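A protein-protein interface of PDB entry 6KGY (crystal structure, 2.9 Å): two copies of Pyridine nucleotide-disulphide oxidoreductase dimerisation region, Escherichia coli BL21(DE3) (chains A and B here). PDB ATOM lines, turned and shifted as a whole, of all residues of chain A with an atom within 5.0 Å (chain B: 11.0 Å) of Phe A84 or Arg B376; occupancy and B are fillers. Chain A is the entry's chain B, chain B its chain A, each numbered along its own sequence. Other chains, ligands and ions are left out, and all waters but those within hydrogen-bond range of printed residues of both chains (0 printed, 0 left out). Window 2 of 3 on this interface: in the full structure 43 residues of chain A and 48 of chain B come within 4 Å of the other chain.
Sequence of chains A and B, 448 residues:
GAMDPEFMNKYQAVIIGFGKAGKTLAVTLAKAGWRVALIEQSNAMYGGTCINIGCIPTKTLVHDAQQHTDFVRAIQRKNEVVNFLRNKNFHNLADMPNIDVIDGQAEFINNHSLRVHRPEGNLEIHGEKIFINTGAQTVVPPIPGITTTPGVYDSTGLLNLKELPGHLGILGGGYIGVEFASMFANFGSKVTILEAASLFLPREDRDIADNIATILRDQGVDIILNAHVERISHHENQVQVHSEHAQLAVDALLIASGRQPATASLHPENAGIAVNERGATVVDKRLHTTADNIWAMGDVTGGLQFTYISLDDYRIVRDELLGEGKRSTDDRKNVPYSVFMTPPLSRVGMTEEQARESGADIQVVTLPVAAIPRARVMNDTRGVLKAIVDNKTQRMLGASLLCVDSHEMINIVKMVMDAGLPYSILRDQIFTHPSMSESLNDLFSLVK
O of Ala B370 sits at hydrogen-bond distance from NZ of Lys A88.
NH2 of Arg A77 lies within hydrogen-bond range of O of Arg B376, at 2.6 Å.
O of Val B377 sits at hydrogen-bond distance from NH2 of Arg A77, at 2.7 Å.
N of Asn B379 lies close to NH2 of Arg A77 (3.1 Å).
The backbone carbonyl oxygen of Ala B370 lies within hydrogen-bond range of the guanidinium group of Arg B376 (2.5 Å).
Among the printed residues, pairs that only touch across the chains: Thr A60 with Val B377, Arg A77 with Met B378, Phe A84 with Arg B376 and Leu A85 with Pro B373.
Of the printed residues of chain B, Arg A77 touches Arg B376 (2.6 Å), Val B377 (2.7 Å), Met B378 (3.7 Å) and Asn B379 (3.1 Å).
Asn A79 touches none of the printed residues of chain B.
No residue of chain B comes within 4 Å of Val A81.
Val A82 touches none of the printed residues of chain B.
No residue of chain B comes within 4 Å of Asn A83.
Phe A84 touches just one residue of chain B: Arg B376 (3.2 Å).
No residue of chain B comes within 4 Å of Asn A87.
Printed residues of chain A within 4 Å of Ala B370: Lys A88.
Hydrophobic or aromatic side chains of chain B that line the printed part of chain A: Pro B373 and Val B377.
Among the printed residues, no Asp or Glu carboxylate lies within 4 Å of a Lys or Arg side-chain nitrogen of the other chain.
No position is printed for both chains.
Of the 8 pairs that touch across the chains among the printed residues, none has its exchanged pair printed and touching as well.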
ATOM      1  N   THR A  60     -11.998  15.787 -17.949  1.00  0.00           N
ATOM      2  CA  THR A  60     -11.282  16.585 -18.939  1.00  0.00           C
ATOM      3  C   THR A  60     -12.037  16.631 -20.262  1.00  0.00           C
ATOM      4  O   THR A  60     -12.045  17.663 -20.944  1.00  0.00           O
ATOM      5  CB  THR A  60      -9.872  16.029 -19.142  1.00  0.00           C
ATOM      6  OG1 THR A  60      -9.227  15.887 -17.870  1.00  0.00           O
ATOM      7  CG2 THR A  60      -9.047  16.965 -20.014  1.00  0.00           C
ATOM      8  N   ARG A  77      -5.803  15.751 -25.876  1.00  0.00           N
ATOM      9  CA  ARG A  77      -5.552  16.557 -24.687  1.00  0.00           C
ATOM     10  C   ARG A  77      -5.785  15.747 -23.418  1.00  0.00           C
ATOM     11  O   ARG A  77      -5.070  15.920 -22.424  1.00  0.00           O
ATOM     12  CB  ARG A  77      -6.436  17.804 -24.695  1.00  0.00           C
ATOM     13  CG  ARG A  77      -6.110  18.796 -23.589  1.00  0.00           C
ATOM     14  CD  ARG A  77      -7.365  19.449 -23.032  1.00  0.00           C
ATOM     15  NE  ARG A  77      -7.218  19.791 -21.621  1.00  0.00           N
ATOM     16  CZ  ARG A  77      -8.182  20.321 -20.876  1.00  0.00           C
ATOM     17  NH1 ARG A  77      -9.370  20.575 -21.406  1.00  0.00           N
ATOM     18  NH2 ARG A  77      -7.956  20.600 -19.599  1.00  0.00           N
ATOM     19  N   ASN A  79      -5.271  12.502 -23.004  1.00  0.00           N
ATOM     20  CA  ASN A  79      -4.162  11.576 -22.793  1.00  0.00           C
ATOM     21  C   ASN A  79      -2.987  12.262 -22.109  1.00  0.00           C
ATOM     22  O   ASN A  79      -2.390  11.707 -21.179  1.00  0.00           O
ATOM     23  CB  ASN A  79      -3.722  10.969 -24.125  1.00  0.00           C
ATOM     24  CG  ASN A  79      -4.823  10.171 -24.797  1.00  0.00           C
ATOM     25  OD1 ASN A  79      -5.587   9.469 -24.136  1.00  0.00           O
ATOM     26  ND2 ASN A  79      -4.907  10.275 -26.118  1.00  0.00           N
ATOM     27  N   GLU A  80      -2.640  13.474 -22.547  1.00  0.00           N
ATOM     28  CA  GLU A  80      -1.478  14.146 -21.981  1.00  0.00           C
ATOM     29  C   GLU A  80      -1.727  14.648 -20.565  1.00  0.00           C
ATOM     30  O   GLU A  80      -0.765  14.844 -19.814  1.00  0.00           O
ATOM     31  CB  GLU A  80      -1.043  15.299 -22.885  1.00  0.00           C
ATOM     32  CG  GLU A  80      -0.461  14.849 -24.222  1.00  0.00           C
ATOM     33  CD  GLU A  80       0.590  13.757 -24.077  1.00  0.00           C
ATOM     34  OE1 GLU A  80       1.400  13.818 -23.127  1.00  0.00           O
ATOM     35  OE2 GLU A  80       0.604  12.834 -24.919  1.00  0.00           O
ATOM     36  N   VAL A  81      -2.987  14.856 -20.179  1.00  0.00           N
ATOM     37  CA  VAL A  81      -3.278  15.205 -18.792  1.00  0.00           C
ATOM     38  C   VAL A  81      -3.047  14.004 -17.884  1.00  0.00           C
ATOM     39  O   VAL A  81      -2.433  14.125 -16.816  1.00  0.00           O
ATOM     40  CB  VAL A  81      -4.712  15.747 -18.657  1.00  0.00           C
ATOM     41  CG1 VAL A  81      -5.065  15.949 -17.190  1.00  0.00           C
ATOM     42  CG2 VAL A  81      -4.860  17.050 -19.423  1.00  0.00           C
ATOM     43  N   VAL A  82      -3.522  12.825 -18.292  1.00  0.00           N
ATOM     44  CA  VAL A  82      -3.327  11.640 -17.464  1.00  0.00           C
ATOM     45  C   VAL A  82      -1.862  11.225 -17.464  1.00  0.00           C
ATOM     46  O   VAL A  82      -1.337  10.773 -16.442  1.00  0.00           O
ATOM     47  CB  VAL A  82      -4.259  10.494 -17.914  1.00  0.00           C
ATOM     48  CG1 VAL A  82      -5.651  11.026 -18.213  1.00  0.00           C
ATOM     49  CG2 VAL A  82      -3.700   9.740 -19.118  1.00  0.00           C
ATOM     50  N   ASN A  83      -1.166  11.404 -18.592  1.00  0.00           N
ATOM     51  CA  ASN A  83       0.236  11.003 -18.655  1.00  0.00           C
ATOM     52  C   ASN A  83       1.121  11.940 -17.844  1.00  0.00           C
ATOM     53  O   ASN A  83       2.158  11.514 -17.324  1.00  0.00           O
ATOM     54  CB  ASN A  83       0.708  10.937 -20.107  1.00  0.00           C
ATOM     55  CG  ASN A  83       0.080   9.783 -20.874  1.00  0.00           C
ATOM     56  OD1 ASN A  83      -0.442   9.965 -21.975  1.00  0.00           O
ATOM     57  ND2 ASN A  83       0.122   8.589 -20.291  1.00  0.00           N
ATOM     58  N   PHE A  84       0.733  13.211 -17.720  1.00  0.00           N
ATOM     59  CA  PHE A  84       1.437  14.106 -16.807  1.00  0.00           C
ATOM     60  C   PHE A  84       1.221  13.676 -15.362  1.00  0.00           C
ATOM     61  O   PHE A  84       2.179  13.400 -14.631  1.00  0.00           O
ATOM     62  CB  PHE A  84       0.970  15.551 -17.015  1.00  0.00           C
ATOM     63  CG  PHE A  84       1.679  16.549 -16.138  1.00  0.00           C
ATOM     64  CD1 PHE A  84       2.752  17.276 -16.624  1.00  0.00           C
ATOM     65  CD2 PHE A  84       1.271  16.760 -14.828  1.00  0.00           C
ATOM     66  CE1 PHE A  84       3.406  18.192 -15.822  1.00  0.00           C
ATOM     67  CE2 PHE A  84       1.925  17.668 -14.022  1.00  0.00           C
ATOM     68  CZ  PHE A  84       2.990  18.389 -14.520  1.00  0.00           C
ATOM     69  N   LEU A  85      -0.044  13.616 -14.935  1.00  0.00           N
ATOM     70  CA  LEU A  85      -0.348  13.306 -13.542  1.00  0.00           C
ATOM     71  C   LEU A  85       0.113  11.907 -13.158  1.00  0.00           C
ATOM     72  O   LEU A  85       0.527  11.685 -12.014  1.00  0.00           O
ATOM     73  CB  LEU A  85      -1.849  13.462 -13.290  1.00  0.00           C
ATOM     74  CG  LEU A  85      -2.397  14.892 -13.276  1.00  0.00           C
ATOM     75  CD1 LEU A  85      -3.864  14.904 -12.875  1.00  0.00           C
ATOM     76  CD2 LEU A  85      -1.577  15.781 -12.351  1.00  0.00           C
ATOM     77  N   ARG A  86       0.049  10.952 -14.091  1.00  0.00           N
ATOM     78  CA  ARG A  86       0.514   9.597 -13.802  1.00  0.00           C
ATOM     79  C   ARG A  86       1.999   9.591 -13.466  1.00  0.00           C
ATOM     80  O   ARG A  86       2.413   9.045 -12.437  1.00  0.00           O
ATOM     81  CB  ARG A  86       0.225   8.680 -14.990  1.00  0.00           C
ATOM     82  CG  ARG A  86       0.522   7.211 -14.754  1.00  0.00           C
ATOM     83  CD  ARG A  86       0.726   6.487 -16.077  1.00  0.00           C
ATOM     84  NE  ARG A  86      -0.536   6.243 -16.771  1.00  0.00           N
ATOM     85  CZ  ARG A  86      -0.628   5.778 -18.013  1.00  0.00           C
ATOM     86  NH1 ARG A  86       0.471   5.507 -18.704  1.00  0.00           N
ATOM     87  NH2 ARG A  86      -1.818   5.585 -18.566  1.00  0.00           N
ATOM     88  N   ASN A  87       2.820  10.191 -14.333  1.00  0.00           N
ATOM     89  CA  ASN A  87       4.245  10.304 -14.045  1.00  0.00           C
ATOM     90  C   ASN A  87       4.493  11.117 -12.782  1.00  0.00           C
ATOM     91  O   ASN A  87       5.446  10.842 -12.043  1.00  0.00           O
ATOM     92  CB  ASN A  87       4.971  10.934 -15.234  1.00  0.00           C
ATOM     93  CG  ASN A  87       6.476  10.939 -15.063  1.00  0.00           C
ATOM     94  OD1 ASN A  87       7.091   9.896 -14.843  1.00  0.00           O
ATOM     95  ND2 ASN A  87       7.079  12.118 -15.162  1.00  0.00           N
ATOM     96  N   LYS A  88       3.648  12.116 -12.519  1.00  0.00           N
ATOM     97  CA  LYS A  88       3.770  12.888 -11.288  1.00  0.00           C
ATOM     98  C   LYS A  88       3.493  12.020 -10.067  1.00  0.00           C
ATOM     99  O   LYS A  88       4.178  12.137  -9.043  1.00  0.00           O
ATOM    100  CB  LYS A  88       2.814  14.081 -11.327  1.00  0.00           C
ATOM    101  CG  LYS A  88       3.015  15.087 -10.206  1.00  0.00           C
ATOM    102  CD  LYS A  88       1.777  15.181  -9.327  1.00  0.00           C
ATOM    103  CE  LYS A  88       1.711  16.518  -8.606  1.00  0.00           C
ATOM    104  NZ  LYS A  88       1.653  17.663  -9.560  1.00  0.00           N
ATOM    105  N   LEU B 367       0.214  27.034  -1.919  1.00  0.00           N
ATOM    106  CA  LEU B 367       0.023  25.814  -2.696  1.00  0.00           C
ATOM    107  C   LEU B 367       0.057  26.178  -4.173  1.00  0.00           C
ATOM    108  O   LEU B 367      -0.732  27.038  -4.615  1.00  0.00           O
ATOM    109  CB  LEU B 367      -1.295  25.123  -2.334  1.00  0.00           C
ATOM    110  CG  LEU B 367      -1.507  23.737  -2.946  1.00  0.00           C
ATOM    111  CD1 LEU B 367      -1.241  22.649  -1.917  1.00  0.00           C
ATOM    112  CD2 LEU B 367      -2.909  23.606  -3.523  1.00  0.00           C
ATOM    113  N   PRO B 368       0.942  25.578  -4.968  1.00  0.00           N
ATOM    114  CA  PRO B 368       0.956  25.871  -6.404  1.00  0.00           C
ATOM    115  C   PRO B 368      -0.250  25.274  -7.111  1.00  0.00           C
ATOM    116  O   PRO B 368      -0.780  24.231  -6.718  1.00  0.00           O
ATOM    117  CB  PRO B 368       2.260  25.224  -6.888  1.00  0.00           C
ATOM    118  CG  PRO B 368       3.082  25.018  -5.646  1.00  0.00           C
ATOM    119  CD  PRO B 368       2.085  24.745  -4.564  1.00  0.00           C
ATOM    120  N   VAL B 369      -0.679  25.953  -8.178  1.00  0.00           N
ATOM    121  CA  VAL B 369      -1.848  25.512  -8.932  1.00  0.00           C
ATOM    122  C   VAL B 369      -1.553  24.281  -9.776  1.00  0.00           C
ATOM    123  O   VAL B 369      -2.486  23.588 -10.198  1.00  0.00           O
ATOM    124  CB  VAL B 369      -2.372  26.646  -9.825  1.00  0.00           C
ATOM    125  CG1 VAL B 369      -3.098  27.688  -8.992  1.00  0.00           C
ATOM    126  CG2 VAL B 369      -1.221  27.263 -10.583  1.00  0.00           C
ATOM    127  N   ALA B 370      -0.279  23.998 -10.051  1.00  0.00           N
ATOM    128  CA  ALA B 370       0.070  22.752 -10.718  1.00  0.00           C
ATOM    129  C   ALA B 370      -0.239  21.533  -9.860  1.00  0.00           C
ATOM    130  O   ALA B 370      -0.255  20.415 -10.384  1.00  0.00           O
ATOM    131  CB  ALA B 370       1.550  22.755 -11.103  1.00  0.00           C
ATOM    132  N   ALA B 371      -0.489  21.727  -8.565  1.00  0.00           N
ATOM    133  CA  ALA B 371      -0.810  20.641  -7.651  1.00  0.00           C
ATOM    134  C   ALA B 371      -2.305  20.380  -7.528  1.00  0.00           C
ATOM    135  O   ALA B 371      -2.693  19.409  -6.869  1.00  0.00           O
ATOM    136  CB  ALA B 371      -0.229  20.935  -6.263  1.00  0.00           C
ATOM    137  N   ILE B 372      -3.148  21.214  -8.131  1.00  0.00           N
ATOM    138  CA  ILE B 372      -4.592  20.999  -8.139  1.00  0.00           C
ATOM    139  C   ILE B 372      -4.940  20.248  -9.422  1.00  0.00           C
ATOM    140  O   ILE B 372      -4.860  20.842 -10.511  1.00  0.00           O
ATOM    141  CB  ILE B 372      -5.364  22.320  -8.048  1.00  0.00           C
ATOM    142  CG1 ILE B 372      -5.027  23.041  -6.746  1.00  0.00           C
ATOM    143  CG2 ILE B 372      -6.862  22.071  -8.144  1.00  0.00           C
ATOM    144  CD1 ILE B 372      -4.671  24.473  -6.948  1.00  0.00           C
ATOM    145  N   PRO B 373      -5.318  18.970  -9.348  1.00  0.00           N
ATOM    146  CA  PRO B 373      -5.672  18.239 -10.574  1.00  0.00           C
ATOM    147  C   PRO B 373      -6.872  18.820 -11.296  1.00  0.00           C
ATOM    148  O   PRO B 373      -7.008  18.610 -12.507  1.00  0.00           O
ATOM    149  CB  PRO B 373      -5.952  16.816 -10.070  1.00  0.00           C
ATOM    150  CG  PRO B 373      -5.299  16.742  -8.715  1.00  0.00           C
ATOM    151  CD  PRO B 373      -5.398  18.121  -8.149  1.00  0.00           C
ATOM    152  N   ARG B 374      -7.748  19.544 -10.594  1.00  0.00           N
ATOM    153  CA  ARG B 374      -8.875  20.191 -11.255  1.00  0.00           C
ATOM    154  C   ARG B 374      -8.416  21.340 -12.144  1.00  0.00           C
ATOM    155  O   ARG B 374      -9.099  21.683 -13.117  1.00  0.00           O
ATOM    156  CB  ARG B 374      -9.880  20.676 -10.208  1.00  0.00           C
ATOM    157  CG  ARG B 374     -11.090  21.415 -10.761  1.00  0.00           C
ATOM    158  CD  ARG B 374     -12.051  20.494 -11.490  1.00  0.00           C
ATOM    159  NE  ARG B 374     -13.197  21.234 -12.011  1.00  0.00           N
ATOM    160  CZ  ARG B 374     -14.095  20.734 -12.852  1.00  0.00           C
ATOM    161  NH1 ARG B 374     -15.104  21.486 -13.272  1.00  0.00           N
ATOM    162  NH2 ARG B 374     -13.986  19.482 -13.274  1.00  0.00           N
ATOM    163  N   ALA B 375      -7.262  21.937 -11.838  1.00  0.00           N
ATOM    164  CA  ALA B 375      -6.739  23.005 -12.684  1.00  0.00           C
ATOM    165  C   ALA B 375      -6.288  22.477 -14.040  1.00  0.00           C
ATOM    166  O   ALA B 375      -6.411  23.181 -15.049  1.00  0.00           O
ATOM    167  CB  ALA B 375      -5.587  23.720 -11.980  1.00  0.00           C
ATOM    168  N   ARG B 376      -5.765  21.249 -14.085  1.00  0.00           N
ATOM    169  CA  ARG B 376      -5.401  20.651 -15.366  1.00  0.00           C
ATOM    170  C   ARG B 376      -6.632  20.228 -16.154  1.00  0.00           C
ATOM    171  O   ARG B 376      -6.592  20.184 -17.389  1.00  0.00           O
ATOM    172  CB  ARG B 376      -4.482  19.449 -15.149  1.00  0.00           C
ATOM    173  CG  ARG B 376      -3.213  19.767 -14.387  1.00  0.00           C
ATOM    174  CD  ARG B 376      -2.027  19.004 -14.954  1.00  0.00           C
ATOM    175  NE  ARG B 376      -0.852  19.857 -15.094  1.00  0.00           N
ATOM    176  CZ  ARG B 376      -0.072  20.226 -14.082  1.00  0.00           C
ATOM    177  NH1 ARG B 376      -0.336  19.809 -12.851  1.00  0.00           N
ATOM    178  NH2 ARG B 376       0.978  21.004 -14.303  1.00  0.00           N
ATOM    179  N   VAL B 377      -7.728  19.912 -15.462  1.00  0.00           N
ATOM    180  CA  VAL B 377      -8.944  19.489 -16.146  1.00  0.00           C
ATOM    181  C   VAL B 377      -9.563  20.647 -16.919  1.00  0.00           C
ATOM    182  O   VAL B 377     -10.137  20.447 -17.997  1.00  0.00           O
ATOM    183  CB  VAL B 377      -9.931  18.885 -15.128  1.00  0.00           C
ATOM    184  CG1 VAL B 377     -11.266  18.586 -15.783  1.00  0.00           C
ATOM    185  CG2 VAL B 377      -9.346  17.624 -14.511  1.00  0.00           C
ATOM    186  N   MET B 378      -9.443  21.869 -16.405  1.00  0.00           N
ATOM    187  CA  MET B 378     -10.030  23.042 -17.039  1.00  0.00           C
ATOM    188  C   MET B 378      -9.048  23.802 -17.921  1.00  0.00           C
ATOM    189  O   MET B 378      -9.397  24.874 -18.428  1.00  0.00           O
ATOM    190  CB  MET B 378     -10.603  23.979 -15.972  1.00  0.00           C
ATOM    191  CG  MET B 378     -11.645  23.322 -15.083  1.00  0.00           C
ATOM    192  SD  MET B 378     -12.787  24.503 -14.348  1.00  0.00           S
ATOM    193  CE  MET B 378     -12.306  24.401 -12.627  1.00  0.00           C
ATOM    194  N   ASN B 379      -7.833  23.281 -18.106  1.00  0.00           N
ATOM    195  CA  ASN B 379      -6.839  23.860 -19.016  1.00  0.00           C
ATOM    196  C   ASN B 379      -6.443  25.275 -18.592  1.00  0.00           C
ATOM    197  O   ASN B 379      -6.432  26.210 -19.396  1.00  0.00           O
ATOM    198  CB  ASN B 379      -7.342  23.840 -20.463  1.00  0.00           C
ATOM    199  CG  ASN B 379      -6.247  23.499 -21.455  1.00  0.00           C
ATOM    200  OD1 ASN B 379      -5.182  23.012 -21.078  1.00  0.00           O
ATOM    201  ND2 ASN B 379      -6.505  23.756 -22.731  1.00  0.00           N
ATOM    202  N   ASP B 380      -6.109  25.427 -17.308  1.00  0.00           N
ATOM    203  CA  ASP B 380      -5.576  26.692 -16.801  1.00  0.00           C
ATOM    204  C   ASP B 380      -4.882  26.395 -15.471  1.00  0.00           C
ATOM    205  O   ASP B 380      -5.550  26.225 -14.448  1.00  0.00           O
ATOM    206  CB  ASP B 380      -6.667  27.737 -16.639  1.00  0.00           C
ATOM    207  CG  ASP B 380      -6.124  29.155 -16.672  1.00  0.00           C
ATOM    208  OD1 ASP B 380      -4.886  29.318 -16.616  1.00  0.00           O
ATOM    209  OD2 ASP B 380      -6.930  30.103 -16.756  1.00  0.00           O
ATOM    210  N   THR B 381      -3.551  26.339 -15.501  1.00  0.00           N
ATOM    211  CA  THR B 381      -2.775  26.032 -14.307  1.00  0.00           C
ATOM    212  C   THR B 381      -1.870  27.197 -13.927  1.00  0.00           C
ATOM    213  O   THR B 381      -0.655  27.026 -13.785  1.00  0.00           O
ATOM    214  CB  THR B 381      -1.943  24.765 -14.520  1.00  0.00           C
ATOM    215  OG1 THR B 381      -1.119  24.921 -15.682  1.00  0.00           O
ATOM    216  CG2 THR B 381      -2.850  23.558 -14.711  1.00  0.00           C
ATOM    217  N   ARG B 382      -2.452  28.382 -13.758  1.00  0.00           N
ATOM    218  CA  ARG B 382      -1.717  29.570 -13.347  1.00  0.00           C
ATOM    219  C   ARG B 382      -2.265  30.089 -12.025  1.00  0.00           C
ATOM    220  O   ARG B 382      -3.450  29.930 -11.718  1.00  0.00           O
ATOM    221  CB  ARG B 382      -1.806  30.684 -14.396  1.00  0.00           C
ATOM    222  CG  ARG B 382      -1.287  30.311 -15.768  1.00  0.00           C
ATOM    223  CD  ARG B 382      -1.756  31.326 -16.795  1.00  0.00           C
ATOM    224  NE  ARG B 382      -3.204  31.282 -16.972  1.00  0.00           N
ATOM    225  CZ  ARG B 382      -3.900  32.167 -17.676  1.00  0.00           C
ATOM    226  NH1 ARG B 382      -3.281  33.178 -18.270  1.00  0.00           N
ATOM    227  NH2 ARG B 382      -5.216  32.046 -17.782  1.00  0.00           N
ATOM    228  N   GLY B 383      -1.390  30.707 -11.246  1.00  0.00           N
ATOM    229  CA  GLY B 383      -1.782  31.378 -10.025  1.00  0.00           C
ATOM    230  C   GLY B 383      -1.243  30.689  -8.785  1.00  0.00           C
ATOM    231  O   GLY B 383      -0.428  29.764  -8.843  1.00  0.00           O
ATOM    232  N   LEU B 385      -2.366  29.748  -4.410  1.00  0.00           N
ATOM    233  CA  LEU B 385      -3.328  29.675  -3.315  1.00  0.00           C
ATOM    234  C   LEU B 385      -2.573  29.964  -2.028  1.00  0.00           C
ATOM    235  O   LEU B 385      -1.749  29.155  -1.588  1.00  0.00           O
ATOM    236  CB  LEU B 385      -4.023  28.316  -3.262  1.00  0.00           C
ATOM    237  CG  LEU B 385      -5.053  28.086  -4.368  1.00  0.00           C
ATOM    238  CD1 LEU B 385      -4.360  27.615  -5.624  1.00  0.00           C
ATOM    239  CD2 LEU B 385      -6.120  27.095  -3.930  1.00  0.00           C
ATOM    240  N   CYS B 403      -6.797  31.548  -8.893  1.00  0.00           N
ATOM    241  CA  CYS B 403      -6.926  30.325  -9.680  1.00  0.00           C
ATOM    242  C   CYS B 403      -8.328  30.295 -10.278  1.00  0.00           C
ATOM    243  O   CYS B 403      -9.102  31.248 -10.146  1.00  0.00           O
ATOM    244  CB  CYS B 403      -6.653  29.081  -8.831  1.00  0.00           C
ATOM    245  SG  CYS B 403      -7.587  29.020  -7.288  1.00  0.00           S
ATOM    246  N   VAL B 404      -8.648  29.182 -10.941  1.00  0.00           N
ATOM    247  CA  VAL B 404      -9.956  29.031 -11.566  1.00  0.00           C
ATOM    248  C   VAL B 404     -11.031  28.930 -10.494  1.00  0.00           C
ATOM    249  O   VAL B 404     -10.856  28.251  -9.472  1.00  0.00           O
ATOM    250  CB  VAL B 404      -9.973  27.799 -12.487  1.00  0.00           C
ATOM    251  CG1 VAL B 404     -11.210  27.819 -13.375  1.00  0.00           C
ATOM    252  CG2 VAL B 404      -8.708  27.745 -13.329  1.00  0.00           C
ATOM    253  N   ASP B 405     -12.151  29.620 -10.722  1.00  0.00           N
ATOM    254  CA  ASP B 405     -13.310  29.591  -9.828  1.00  0.00           C
ATOM    255  C   ASP B 405     -12.955  30.039  -8.412  1.00  0.00           C
ATOM    256  O   ASP B 405     -13.592  29.622  -7.442  1.00  0.00           O
ATOM    257  CB  ASP B 405     -13.956  28.202  -9.799  1.00  0.00           C
ATOM    258  CG  ASP B 405     -14.543  27.806 -11.138  1.00  0.00           C
ATOM    259  OD1 ASP B 405     -14.515  26.601 -11.467  1.00  0.00           O
ATOM    260  OD2 ASP B 405     -15.032  28.699 -11.862  1.00  0.00           O
ATOM    261  N   PRO B 434     -13.984  15.772  -8.792  1.00  0.00           N
ATOM    262  CA  PRO B 434     -12.873  16.711  -8.621  1.00  0.00           C
ATOM    263  C   PRO B 434     -13.337  18.161  -8.641  1.00  0.00           C
ATOM    264  O   PRO B 434     -14.232  18.518  -9.407  1.00  0.00           O
ATOM    265  CB  PRO B 434     -11.968  16.410  -9.821  1.00  0.00           C
ATOM    266  CG  PRO B 434     -12.814  15.612 -10.783  1.00  0.00           C
ATOM    267  CD  PRO B 434     -14.189  15.440 -10.207  1.00  0.00           C
ATOM    268  N   SER B 435     -12.719  18.991  -7.807  1.00  0.00           N
ATOM    269  CA  SER B 435     -13.162  20.365  -7.642  1.00  0.00           C
ATOM    270  C   SER B 435     -11.964  21.247  -7.326  1.00  0.00           C
ATOM    271  O   SER B 435     -10.854  20.767  -7.086  1.00  0.00           O
ATOM    272  CB  SER B 435     -14.220  20.471  -6.539  1.00  0.00           C
ATOM    273  OG  SER B 435     -14.637  21.810  -6.358  1.00  0.00           O
ATOM    274  N   MET B 436     -12.205  22.556  -7.342  1.00  0.00           N
ATOM    275  CA  MET B 436     -11.207  23.517  -6.896  1.00  0.00           C
ATOM    276  C   MET B 436     -11.304  23.793  -5.404  1.00  0.00           C
ATOM    277  O   MET B 436     -10.292  24.124  -4.775  1.00  0.00           O
ATOM    278  CB  MET B 436     -11.353  24.831  -7.670  1.00  0.00           C
ATOM    279  CG  MET B 436     -11.197  24.696  -9.175  1.00  0.00           C
ATOM    280  SD  MET B 436      -9.506  24.328  -9.686  1.00  0.00           S
ATOM    281  CE  MET B 436      -8.661  25.835  -9.216  1.00  0.00           C
ATOM    282  N   GLU B 438     -11.792  21.611  -3.113  1.00  0.00           N
ATOM    283  CA  GLU B 438     -11.093  20.556  -2.389  1.00  0.00           C
ATOM    284  C   GLU B 438      -9.591  20.794  -2.312  1.00  0.00           C
ATOM    285  O   GLU B 438      -8.905  20.058  -1.596  1.00  0.00           O
ATOM    286  CB  GLU B 438     -11.369  19.196  -3.031  1.00  0.00           C
ATOM    287  CG  GLU B 438     -10.723  18.993  -4.384  1.00  0.00           C
ATOM    288  CD  GLU B 438     -10.917  17.585  -4.905  1.00  0.00           C
ATOM    289  OE1 GLU B 438     -10.925  17.403  -6.140  1.00  0.00           O
ATOM    290  OE2 GLU B 438     -11.060  16.660  -4.078  1.00  0.00           O
ATOM    291  N   SER B 439      -9.066  21.792  -3.030  1.00  0.00           N
ATOM    292  CA  SER B 439      -7.662  22.153  -2.871  1.00  0.00           C
ATOM    293  C   SER B 439      -7.366  22.606  -1.449  1.00  0.00           C
ATOM    294  O   SER B 439      -6.223  22.499  -0.988  1.00  0.00           O
ATOM    295  CB  SER B 439      -7.282  23.251  -3.865  1.00  0.00           C
ATOM    296  OG  SER B 439      -7.944  23.073  -5.106  1.00  0.00           O
